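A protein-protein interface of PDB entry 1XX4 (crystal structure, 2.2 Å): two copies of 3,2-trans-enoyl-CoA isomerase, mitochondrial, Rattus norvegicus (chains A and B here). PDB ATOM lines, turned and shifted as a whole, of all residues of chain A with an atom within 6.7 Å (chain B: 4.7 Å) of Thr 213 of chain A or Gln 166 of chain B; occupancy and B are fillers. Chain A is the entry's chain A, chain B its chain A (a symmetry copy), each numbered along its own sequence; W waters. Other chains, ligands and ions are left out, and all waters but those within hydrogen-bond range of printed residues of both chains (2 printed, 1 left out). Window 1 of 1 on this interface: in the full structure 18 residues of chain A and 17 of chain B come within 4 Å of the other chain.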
ATOM      1  N   LEU A  99      16.646 -20.851   7.948  1.00  0.00           N
ATOM      2  CA  LEU A  99      17.943 -21.506   7.898  1.00  0.00           C
ATOM      3  C   LEU A  99      18.430 -21.668   9.324  1.00  0.00           C
ATOM      4  O   LEU A  99      17.953 -20.975  10.223  1.00  0.00           O
ATOM      5  CB  LEU A  99      18.952 -20.630   7.156  1.00  0.00           C
ATOM      6  CG  LEU A  99      18.864 -20.438   5.645  1.00  0.00           C
ATOM      7  CD1 LEU A  99      19.738 -19.254   5.235  1.00  0.00           C
ATOM      8  CD2 LEU A  99      19.320 -21.707   4.935  1.00  0.00           C
ATOM      9  N   THR A 100      19.363 -22.589   9.540  1.00  0.00           N
ATOM     10  CA  THR A 100      19.944 -22.739  10.859  1.00  0.00           C
ATOM     11  C   THR A 100      21.121 -21.776  10.805  1.00  0.00           C
ATOM     12  O   THR A 100      21.992 -21.911   9.946  1.00  0.00           O
ATOM     13  CB  THR A 100      20.478 -24.159  11.124  1.00  0.00           C
ATOM     14  OG1 THR A 100      19.383 -25.040  11.380  1.00  0.00           O
ATOM     15  CG2 THR A 100      21.391 -24.170  12.336  1.00  0.00           C
ATOM     16  N   ASP A 121      20.919 -19.255  15.956  1.00  0.00           N
ATOM     17  CA  ASP A 121      20.414 -20.419  16.681  1.00  0.00           C
ATOM     18  C   ASP A 121      21.481 -20.997  17.594  1.00  0.00           C
ATOM     19  O   ASP A 121      21.194 -21.853  18.431  1.00  0.00           O
ATOM     20  CB  ASP A 121      19.974 -21.504  15.698  1.00  0.00           C
ATOM     21  CG  ASP A 121      18.811 -21.065  14.834  1.00  0.00           C
ATOM     22  OD1 ASP A 121      17.806 -20.582  15.398  1.00  0.00           O
ATOM     23  OD2 ASP A 121      18.890 -21.205  13.595  1.00  0.00           O
ATOM     24  N   TRP A 202      22.720 -29.988  13.811  1.00  0.00           N
ATOM     25  CA  TRP A 202      21.421 -29.390  13.559  1.00  0.00           C
ATOM     26  C   TRP A 202      20.819 -29.940  12.283  1.00  0.00           C
ATOM     27  O   TRP A 202      19.599 -29.979  12.130  1.00  0.00           O
ATOM     28  CB  TRP A 202      21.524 -27.862  13.476  1.00  0.00           C
ATOM     29  CG  TRP A 202      21.670 -27.214  14.814  1.00  0.00           C
ATOM     30  CD1 TRP A 202      22.736 -27.320  15.660  1.00  0.00           C
ATOM     31  CD2 TRP A 202      20.689 -26.438  15.503  1.00  0.00           C
ATOM     32  NE1 TRP A 202      22.478 -26.664  16.839  1.00  0.00           N
ATOM     33  CE2 TRP A 202      21.226 -26.112  16.771  1.00  0.00           C
ATOM     34  CE3 TRP A 202      19.405 -25.986  15.178  1.00  0.00           C
ATOM     35  CZ2 TRP A 202      20.526 -25.357  17.717  1.00  0.00           C
ATOM     36  CZ3 TRP A 202      18.702 -25.231  16.121  1.00  0.00           C
ATOM     37  CH2 TRP A 202      19.269 -24.926  17.377  1.00  0.00           C
ATOM     38  N   ILE A 205      18.336 -32.823  12.200  1.00  0.00           N
ATOM     39  CA  ILE A 205      16.962 -32.504  12.567  1.00  0.00           C
ATOM     40  C   ILE A 205      16.118 -32.255  11.320  1.00  0.00           C
ATOM     41  O   ILE A 205      16.461 -31.417  10.480  1.00  0.00           O
ATOM     42  CB  ILE A 205      16.897 -31.227  13.440  1.00  0.00           C
ATOM     43  CG1 ILE A 205      17.869 -31.337  14.615  1.00  0.00           C
ATOM     44  CG2 ILE A 205      15.470 -31.001  13.924  1.00  0.00           C
ATOM     45  CD1 ILE A 205      17.549 -32.434  15.595  1.00  0.00           C
ATOM     46  N   PRO A 206      14.997 -32.977  11.180  1.00  0.00           N
ATOM     47  CA  PRO A 206      14.159 -32.757   9.997  1.00  0.00           C
ATOM     48  C   PRO A 206      13.795 -31.282   9.843  1.00  0.00           C
ATOM     49  O   PRO A 206      13.172 -30.690  10.725  1.00  0.00           O
ATOM     50  CB  PRO A 206      12.950 -33.668  10.244  1.00  0.00           C
ATOM     51  CG  PRO A 206      12.988 -33.947  11.743  1.00  0.00           C
ATOM     52  CD  PRO A 206      14.450 -34.044  12.036  1.00  0.00           C
ATOM     53  N   HIS A 208      11.537 -29.297   8.268  1.00  0.00           N
ATOM     54  CA  HIS A 208      10.205 -28.741   8.497  1.00  0.00           C
ATOM     55  C   HIS A 208       9.818 -28.571   9.969  1.00  0.00           C
ATOM     56  O   HIS A 208       9.305 -27.521  10.359  1.00  0.00           O
ATOM     57  CB  HIS A 208       9.147 -29.577   7.766  1.00  0.00           C
ATOM     58  CG  HIS A 208       8.948 -30.943   8.345  1.00  0.00           C
ATOM     59  ND1 HIS A 208       7.809 -31.298   9.036  1.00  0.00           N
ATOM     60  CD2 HIS A 208       9.744 -32.039   8.342  1.00  0.00           C
ATOM     61  CE1 HIS A 208       7.911 -32.555   9.433  1.00  0.00           C
ATOM     62  NE2 HIS A 208       9.076 -33.026   9.025  1.00  0.00           N
ATOM     63  N   SER A 209      10.063 -29.592  10.784  1.00  0.00           N
ATOM     64  CA  SER A 209       9.725 -29.503  12.206  1.00  0.00           C
ATOM     65  C   SER A 209      10.673 -28.558  12.953  1.00  0.00           C
ATOM     66  O   SER A 209      10.269 -27.899  13.910  1.00  0.00           O
ATOM     67  CB  SER A 209       9.728 -30.890  12.856  1.00  0.00           C
ATOM     68  OG  SER A 209      10.971 -31.534  12.672  1.00  0.00           O
ATOM     69  N   ARG A 210      11.927 -28.482  12.518  1.00  0.00           N
ATOM     70  CA  ARG A 210      12.872 -27.570  13.159  1.00  0.00           C
ATOM     71  C   ARG A 210      12.417 -26.145  12.901  1.00  0.00           C
ATOM     72  O   ARG A 210      12.369 -25.309  13.805  1.00  0.00           O
ATOM     73  CB  ARG A 210      14.281 -27.736  12.596  1.00  0.00           C
ATOM     74  CG  ARG A 210      15.254 -26.664  13.088  1.00  0.00           C
ATOM     75  CD  ARG A 210      16.639 -26.824  12.477  1.00  0.00           C
ATOM     76  NE  ARG A 210      16.605 -26.703  11.021  1.00  0.00           N
ATOM     77  CZ  ARG A 210      16.345 -25.576  10.365  1.00  0.00           C
ATOM     78  NH1 ARG A 210      16.099 -24.461  11.033  1.00  0.00           N
ATOM     79  NH2 ARG A 210      16.322 -25.569   9.040  1.00  0.00           N
ATOM     80  N   GLN A 211      12.073 -25.881  11.650  1.00  0.00           N
ATOM     81  CA  GLN A 211      11.633 -24.562  11.238  1.00  0.00           C
ATOM     82  C   GLN A 211      10.328 -24.105  11.890  1.00  0.00           C
ATOM     83  O   GLN A 211      10.180 -22.925  12.229  1.00  0.00           O
ATOM     84  CB  GLN A 211      11.516 -24.531   9.717  1.00  0.00           C
ATOM     85  CG  GLN A 211      12.855 -24.715   9.032  1.00  0.00           C
ATOM     86  CD  GLN A 211      12.726 -24.814   7.529  1.00  0.00           C
ATOM     87  OE1 GLN A 211      13.700 -24.622   6.798  1.00  0.00           O
ATOM     88  NE2 GLN A 211      11.529 -25.126   7.057  1.00  0.00           N
ATOM     89  N   LEU A 212       9.384 -25.026  12.061  1.00  0.00           N
ATOM     90  CA  LEU A 212       8.112 -24.694  12.696  1.00  0.00           C
ATOM     91  C   LEU A 212       8.331 -24.416  14.182  1.00  0.00           C
ATOM     92  O   LEU A 212       7.689 -23.533  14.767  1.00  0.00           O
ATOM     93  CB  LEU A 212       7.114 -25.838  12.529  1.00  0.00           C
ATOM     94  CG  LEU A 212       6.488 -25.938  11.142  1.00  0.00           C
ATOM     95  CD1 LEU A 212       5.624 -27.197  11.046  1.00  0.00           C
ATOM     96  CD2 LEU A 212       5.662 -24.678  10.884  1.00  0.00           C
ATOM     97  N   THR A 213       9.235 -25.180  14.786  1.00  0.00           N
ATOM     98  CA  THR A 213       9.548 -25.006  16.190  1.00  0.00           C
ATOM     99  C   THR A 213      10.156 -23.618  16.376  1.00  0.00           C
ATOM    100  O   THR A 213       9.703 -22.824  17.210  1.00  0.00           O
ATOM    101  CB  THR A 213      10.542 -26.072  16.655  1.00  0.00           C
ATOM    102  OG1 THR A 213       9.923 -27.359  16.571  1.00  0.00           O
ATOM    103  CG2 THR A 213      10.976 -25.817  18.086  1.00  0.00           C
ATOM    104  N   LYS A 214      11.173 -23.329  15.572  1.00  0.00           N
ATOM    105  CA  LYS A 214      11.858 -22.041  15.639  1.00  0.00           C
ATOM    106  C   LYS A 214      10.854 -20.908  15.461  1.00  0.00           C
ATOM    107  O   LYS A 214      10.792 -19.983  16.273  1.00  0.00           O
ATOM    108  CB  LYS A 214      12.941 -21.957  14.553  1.00  0.00           C
ATOM    109  CG  LYS A 214      13.680 -20.621  14.501  1.00  0.00           C
ATOM    110  CD  LYS A 214      14.897 -20.689  13.588  1.00  0.00           C
ATOM    111  CE  LYS A 214      15.644 -19.370  13.568  1.00  0.00           C
ATOM    112  NZ  LYS A 214      16.746 -19.396  12.579  1.00  0.00           N
ATOM    113  N   SER A 215      10.075 -20.986  14.388  1.00  0.00           N
ATOM    114  CA  SER A 215       9.069 -19.979  14.095  1.00  0.00           C
ATOM    115  C   SER A 215       8.185 -19.780  15.319  1.00  0.00           C
ATOM    116  O   SER A 215       7.880 -18.649  15.703  1.00  0.00           O
ATOM    117  CB  SER A 215       8.216 -20.420  12.905  1.00  0.00           C
ATOM    118  OG  SER A 215       7.162 -19.498  12.703  1.00  0.00           O
ATOM    119  N   MET A 216       7.795 -20.892  15.933  1.00  0.00           N
ATOM    120  CA  MET A 216       6.944 -20.881  17.121  1.00  0.00           C
ATOM    121  C   MET A 216       7.574 -20.154  18.304  1.00  0.00           C
ATOM    122  O   MET A 216       6.884 -19.448  19.038  1.00  0.00           O
ATOM    123  CB  MET A 216       6.596 -22.319  17.521  1.00  0.00           C
ATOM    124  CG  MET A 216       6.053 -22.464  18.936  1.00  0.00           C
ATOM    125  SD  MET A 216       5.517 -24.150  19.347  1.00  0.00           S
ATOM    126  CE  MET A 216       7.105 -24.993  19.554  1.00  0.00           C
ATOM    127  N   MET A 217       8.881 -20.338  18.486  1.00  0.00           N
ATOM    128  CA  MET A 217       9.626 -19.705  19.584  1.00  0.00           C
ATOM    129  C   MET A 217       9.771 -18.192  19.434  1.00  0.00           C
ATOM    130  O   MET A 217       9.797 -17.468  20.430  1.00  0.00           O
ATOM    131  CB  MET A 217      11.060 -20.257  19.675  1.00  0.00           C
ATOM    132  CG  MET A 217      11.213 -21.741  19.911  1.00  0.00           C
ATOM    133  SD  MET A 217      10.458 -22.255  21.441  1.00  0.00           S
ATOM    134  CE  MET A 217      11.372 -21.363  22.669  1.00  0.00           C
ATOM    135  N   ARG A 218       9.869 -17.722  18.189  1.00  0.00           N
ATOM    136  CA  ARG A 218      10.119 -16.315  17.925  1.00  0.00           C
ATOM    137  C   ARG A 218       9.040 -15.392  17.361  1.00  0.00           C
ATOM    138  O   ARG A 218       9.219 -14.175  17.379  1.00  0.00           O
ATOM    139  CB  ARG A 218      11.363 -16.226  17.042  1.00  0.00           C
ATOM    140  CG  ARG A 218      12.595 -16.850  17.677  1.00  0.00           C
ATOM    141  CD  ARG A 218      13.770 -16.953  16.708  1.00  0.00           C
ATOM    142  NE  ARG A 218      15.016 -17.225  17.418  1.00  0.00           N
ATOM    143  CZ  ARG A 218      16.230 -17.071  16.897  1.00  0.00           C
ATOM    144  NH1 ARG A 218      17.309 -17.337  17.628  1.00  0.00           N
ATOM    145  NH2 ARG A 218      16.369 -16.649  15.646  1.00  0.00           N
ATOM    146  N   SER B 138      10.402 -32.608  17.522  1.00  0.00           N
ATOM    147  CA  SER B 138      11.054 -32.258  16.263  1.00  0.00           C
ATOM    148  C   SER B 138      11.672 -33.448  15.528  1.00  0.00           C
ATOM    149  O   SER B 138      11.643 -33.510  14.296  1.00  0.00           O
ATOM    150  CB  SER B 138      12.130 -31.203  16.510  1.00  0.00           C
ATOM    151  OG  SER B 138      13.179 -31.723  17.307  1.00  0.00           O
ATOM    152  N   VAL B 143       5.934 -31.202  16.248  1.00  0.00           N
ATOM    153  CA  VAL B 143       6.328 -30.004  16.982  1.00  0.00           C
ATOM    154  C   VAL B 143       5.466 -29.833  18.236  1.00  0.00           C
ATOM    155  O   VAL B 143       4.253 -30.015  18.204  1.00  0.00           O
ATOM    156  CB  VAL B 143       6.248 -28.731  16.087  1.00  0.00           C
ATOM    157  CG1 VAL B 143       5.065 -28.820  15.146  1.00  0.00           C
ATOM    158  CG2 VAL B 143       6.151 -27.483  16.953  1.00  0.00           C
ATOM    159  N   ALA B 161      15.212 -23.560  26.032  1.00  0.00           N
ATOM    160  CA  ALA B 161      14.065 -24.176  25.383  1.00  0.00           C
ATOM    161  C   ALA B 161      14.190 -24.100  23.867  1.00  0.00           C
ATOM    162  O   ALA B 161      13.848 -25.040  23.154  1.00  0.00           O
ATOM    163  CB  ALA B 161      12.781 -23.481  25.825  1.00  0.00           C
ATOM    164  N   GLU B 162      14.678 -22.970  23.378  1.00  0.00           N
ATOM    165  CA  GLU B 162      14.830 -22.769  21.948  1.00  0.00           C
ATOM    166  C   GLU B 162      15.764 -23.834  21.358  1.00  0.00           C
ATOM    167  O   GLU B 162      15.503 -24.385  20.286  1.00  0.00           O
ATOM    168  CB  GLU B 162      15.395 -21.372  21.698  1.00  0.00           C
ATOM    169  CG  GLU B 162      14.897 -20.692  20.439  1.00  0.00           C
ATOM    170  CD  GLU B 162      15.516 -19.311  20.243  1.00  0.00           C
ATOM    171  OE1 GLU B 162      16.755 -19.231  20.075  1.00  0.00           O
ATOM    172  OE2 GLU B 162      14.767 -18.307  20.261  1.00  0.00           O
ATOM    173  N   ARG B 163      16.852 -24.123  22.069  1.00  0.00           N
ATOM    174  CA  ARG B 163      17.810 -25.113  21.609  1.00  0.00           C
ATOM    175  C   ARG B 163      17.260 -26.526  21.764  1.00  0.00           C
ATOM    176  O   ARG B 163      17.241 -27.298  20.813  1.00  0.00           O
ATOM    177  CB  ARG B 163      19.112 -24.985  22.392  1.00  0.00           C
ATOM    178  CG  ARG B 163      20.323 -25.237  21.529  1.00  0.00           C
ATOM    179  CD  ARG B 163      21.222 -26.306  22.101  1.00  0.00           C
ATOM    180  NE  ARG B 163      22.125 -25.802  23.129  1.00  0.00           N
ATOM    181  CZ  ARG B 163      23.176 -26.483  23.576  1.00  0.00           C
ATOM    182  NH1 ARG B 163      23.439 -27.687  23.081  1.00  0.00           N
ATOM    183  NH2 ARG B 163      23.975 -25.958  24.500  1.00  0.00           N
ATOM    184  N   ALA B 164      16.793 -26.847  22.968  1.00  0.00           N
ATOM    185  CA  ALA B 164      16.253 -28.165  23.276  1.00  0.00           C
ATOM    186  C   ALA B 164      15.089 -28.596  22.385  1.00  0.00           C
ATOM    187  O   ALA B 164      15.043 -29.737  21.931  1.00  0.00           O
ATOM    188  CB  ALA B 164      15.843 -28.215  24.735  1.00  0.00           C
ATOM    189  N   LEU B 165      14.144 -27.693  22.142  1.00  0.00           N
ATOM    190  CA  LEU B 165      13.001 -28.016  21.294  1.00  0.00           C
ATOM    191  C   LEU B 165      13.378 -28.233  19.826  1.00  0.00           C
ATOM    192  O   LEU B 165      12.830 -29.120  19.168  1.00  0.00           O
ATOM    193  CB  LEU B 165      11.931 -26.920  21.390  1.00  0.00           C
ATOM    194  CG  LEU B 165      10.988 -26.968  22.600  1.00  0.00           C
ATOM    195  CD1 LEU B 165      10.163 -25.699  22.667  1.00  0.00           C
ATOM    196  CD2 LEU B 165      10.081 -28.188  22.495  1.00  0.00           C
ATOM    197  N   GLN B 166      14.299 -27.424  19.308  1.00  0.00           N
ATOM    198  CA  GLN B 166      14.722 -27.564  17.913  1.00  0.00           C
ATOM    199  C   GLN B 166      15.544 -28.824  17.687  1.00  0.00           C
ATOM    200  O   GLN B 166      15.378 -29.514  16.681  1.00  0.00           O
ATOM    201  CB  GLN B 166      15.534 -26.349  17.478  1.00  0.00           C
ATOM    202  CG  GLN B 166      14.689 -25.138  17.148  1.00  0.00           C
ATOM    203  CD  GLN B 166      15.533 -23.961  16.736  1.00  0.00           C
ATOM    204  OE1 GLN B 166      16.046 -23.231  17.579  1.00  0.00           O
ATOM    205  NE2 GLN B 166      15.700 -23.776  15.430  1.00  0.00           N
ATOM    206  N   LEU B 167      16.432 -29.118  18.629  1.00  0.00           N
ATOM    207  CA  LEU B 167      17.275 -30.304  18.548  1.00  0.00           C
ATOM    208  C   LEU B 167      16.560 -31.508  19.147  1.00  0.00           C
ATOM    209  O   LEU B 167      17.080 -32.615  19.090  1.00  0.00           O
ATOM    210  CB  LEU B 167      18.585 -30.079  19.306  1.00  0.00           C
ATOM    211  CG  LEU B 167      19.571 -29.049  18.749  1.00  0.00           C
ATOM    212  CD1 LEU B 167      20.642 -28.768  19.786  1.00  0.00           C
ATOM    213  CD2 LEU B 167      20.193 -29.561  17.452  1.00  0.00           C
ATOM    214  N   GLY B 168      15.375 -31.291  19.719  1.00  0.00           N
ATOM    215  CA  GLY B 168      14.628 -32.379  20.331  1.00  0.00           C
ATOM    216  C   GLY B 168      15.436 -33.068  21.420  1.00  0.00           C
ATOM    217  O   GLY B 168      15.292 -34.271  21.652  1.00  0.00           O
HETATM  218  O   HOH W   1      17.446 -23.620  13.347  1.00  0.00           O
HETATM  219  O   HOH W   2      18.722 -22.200  19.447  1.00  0.00           O
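OG of Ser 209 of chain A lies within hydrogen-bond range of O of Ser 138 of chain B, at 2.6 Å. NE of Arg 218 of chain A is in salt-bridge range of OE2 of Glu 162 of chain B, 3.1 Å away.
The backbone carbonyl oxygen (O) of Leu 99 of chain A sits at hydrogen-bond distance from the side-chain amino group (NZ) of Lys 214 of chain A. The side-chain hydroxyl (OG1) of Thr 100 of chain A lies close to the guanidinium group (NE) of Arg 210 of chain A (3.3 Å). The side-chain hydroxyl (OG1) of Thr 213 of chain A is in hydrogen-bond range of the backbone carbonyl oxygen (O) of Ser 209 of chain A, 2.7 Å away. OG of Ser 138 of chain B lies within hydrogen-bond range of O of Leu 165 of chain B, at 3.2 Å. N of Gly 168 of chain B lies within hydrogen-bond range of OG of Ser 138 of chain B (3.3 Å). O of Glu 162 of chain B lies close to OE1 of Gln 166 of chain B, at 3.0 Å.
Asp 121 of chain A touches Gln 166 of chain B. Trp 202 of chain A touches Gln 166 of chain B (CZ3 to NE2, 3.4 Å). Ile 205 of chain A touches Gln 166 of chain B. Ile 205 of chain A touches Leu 167 of chain B (CD1 to O, 3.5 Å). Ser 138 of chain B touches Pro 206 of chain A (O to CG, 2.9 Å). Arg 210 of chain A touches Gln 166 of chain B (CG to NE2, 3.7 Å). Thr 213 of chain A touches Val 143 of chain B (OG1 to CG2, 3.8 Å). CB of Leu 165 of chain B touches CG2 of Thr 213 of chain A, 3.6 Å away. Glu 162 of chain B touches Met 217 of chain A. Met 217 of chain A touches Leu 165 of chain B.
Of chain B, only Val 143 (3.8 Å), Leu 165 (3.6 Å) and Gln 166 (3.9 Å) come within 4 Å of Thr 213 of chain A. Of the printed residues of chain B, Lys 214 of chain A touches Gln 166 (3.4 Å). Of the printed residues of chain B, Ile 205 of chain A touches Gln 166 and Leu 167. His 208 of chain A touches none of the printed residues of chain B. Ala 161 of chain B touches none of the printed residues of chain A. The nearest residue of chain B that does not touch Thr 213 of chain A is Ser 138 of chain B (4.4 Å). The nearest printed residue of chain A that does not touch Val 143 of chain B is Leu 212 of chain A (4.4 Å).
Hydrophobic or aromatic side chains of chain A that line the printed part of chain B: Trp 202, Ile 205, Pro 206, Met 216 and Met 217. Of the 10 printed residues of chain B, 7 touch a printed residue of chain A. Printed residues of chain B that touch a printed residue of chain A: Ser 138, Val 143, Glu 162, Arg 163, Leu 165, Gln 166 and Leu 167. Hydrophobic or aromatic side chains of chain B within 4 Å of the printed part of chain A: Val 143, Leu 165 and Leu 167. Among the printed residues, 17 pairs touch across the chains.
No position is printed for both chains. Of the 17 pairs that touch across the chains among the printed residues, none has its exchanged pair printed and touching as well.
Water W2 lies within hydrogen-bond range of O of Asp 121 of chain A (2.7 Å) and OE1 of Gln 166 of chain B (3.4 Å). Water W1 lies within hydrogen-bond range of NE2 of Gln 166 of chain B (2.7 Å), NH1 of Arg 210 of chain A (2.8 Å), OD2 of Asp 121 of chain A (2.8 Å) and OG1 of Thr 100 of chain A (3.1 Å).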
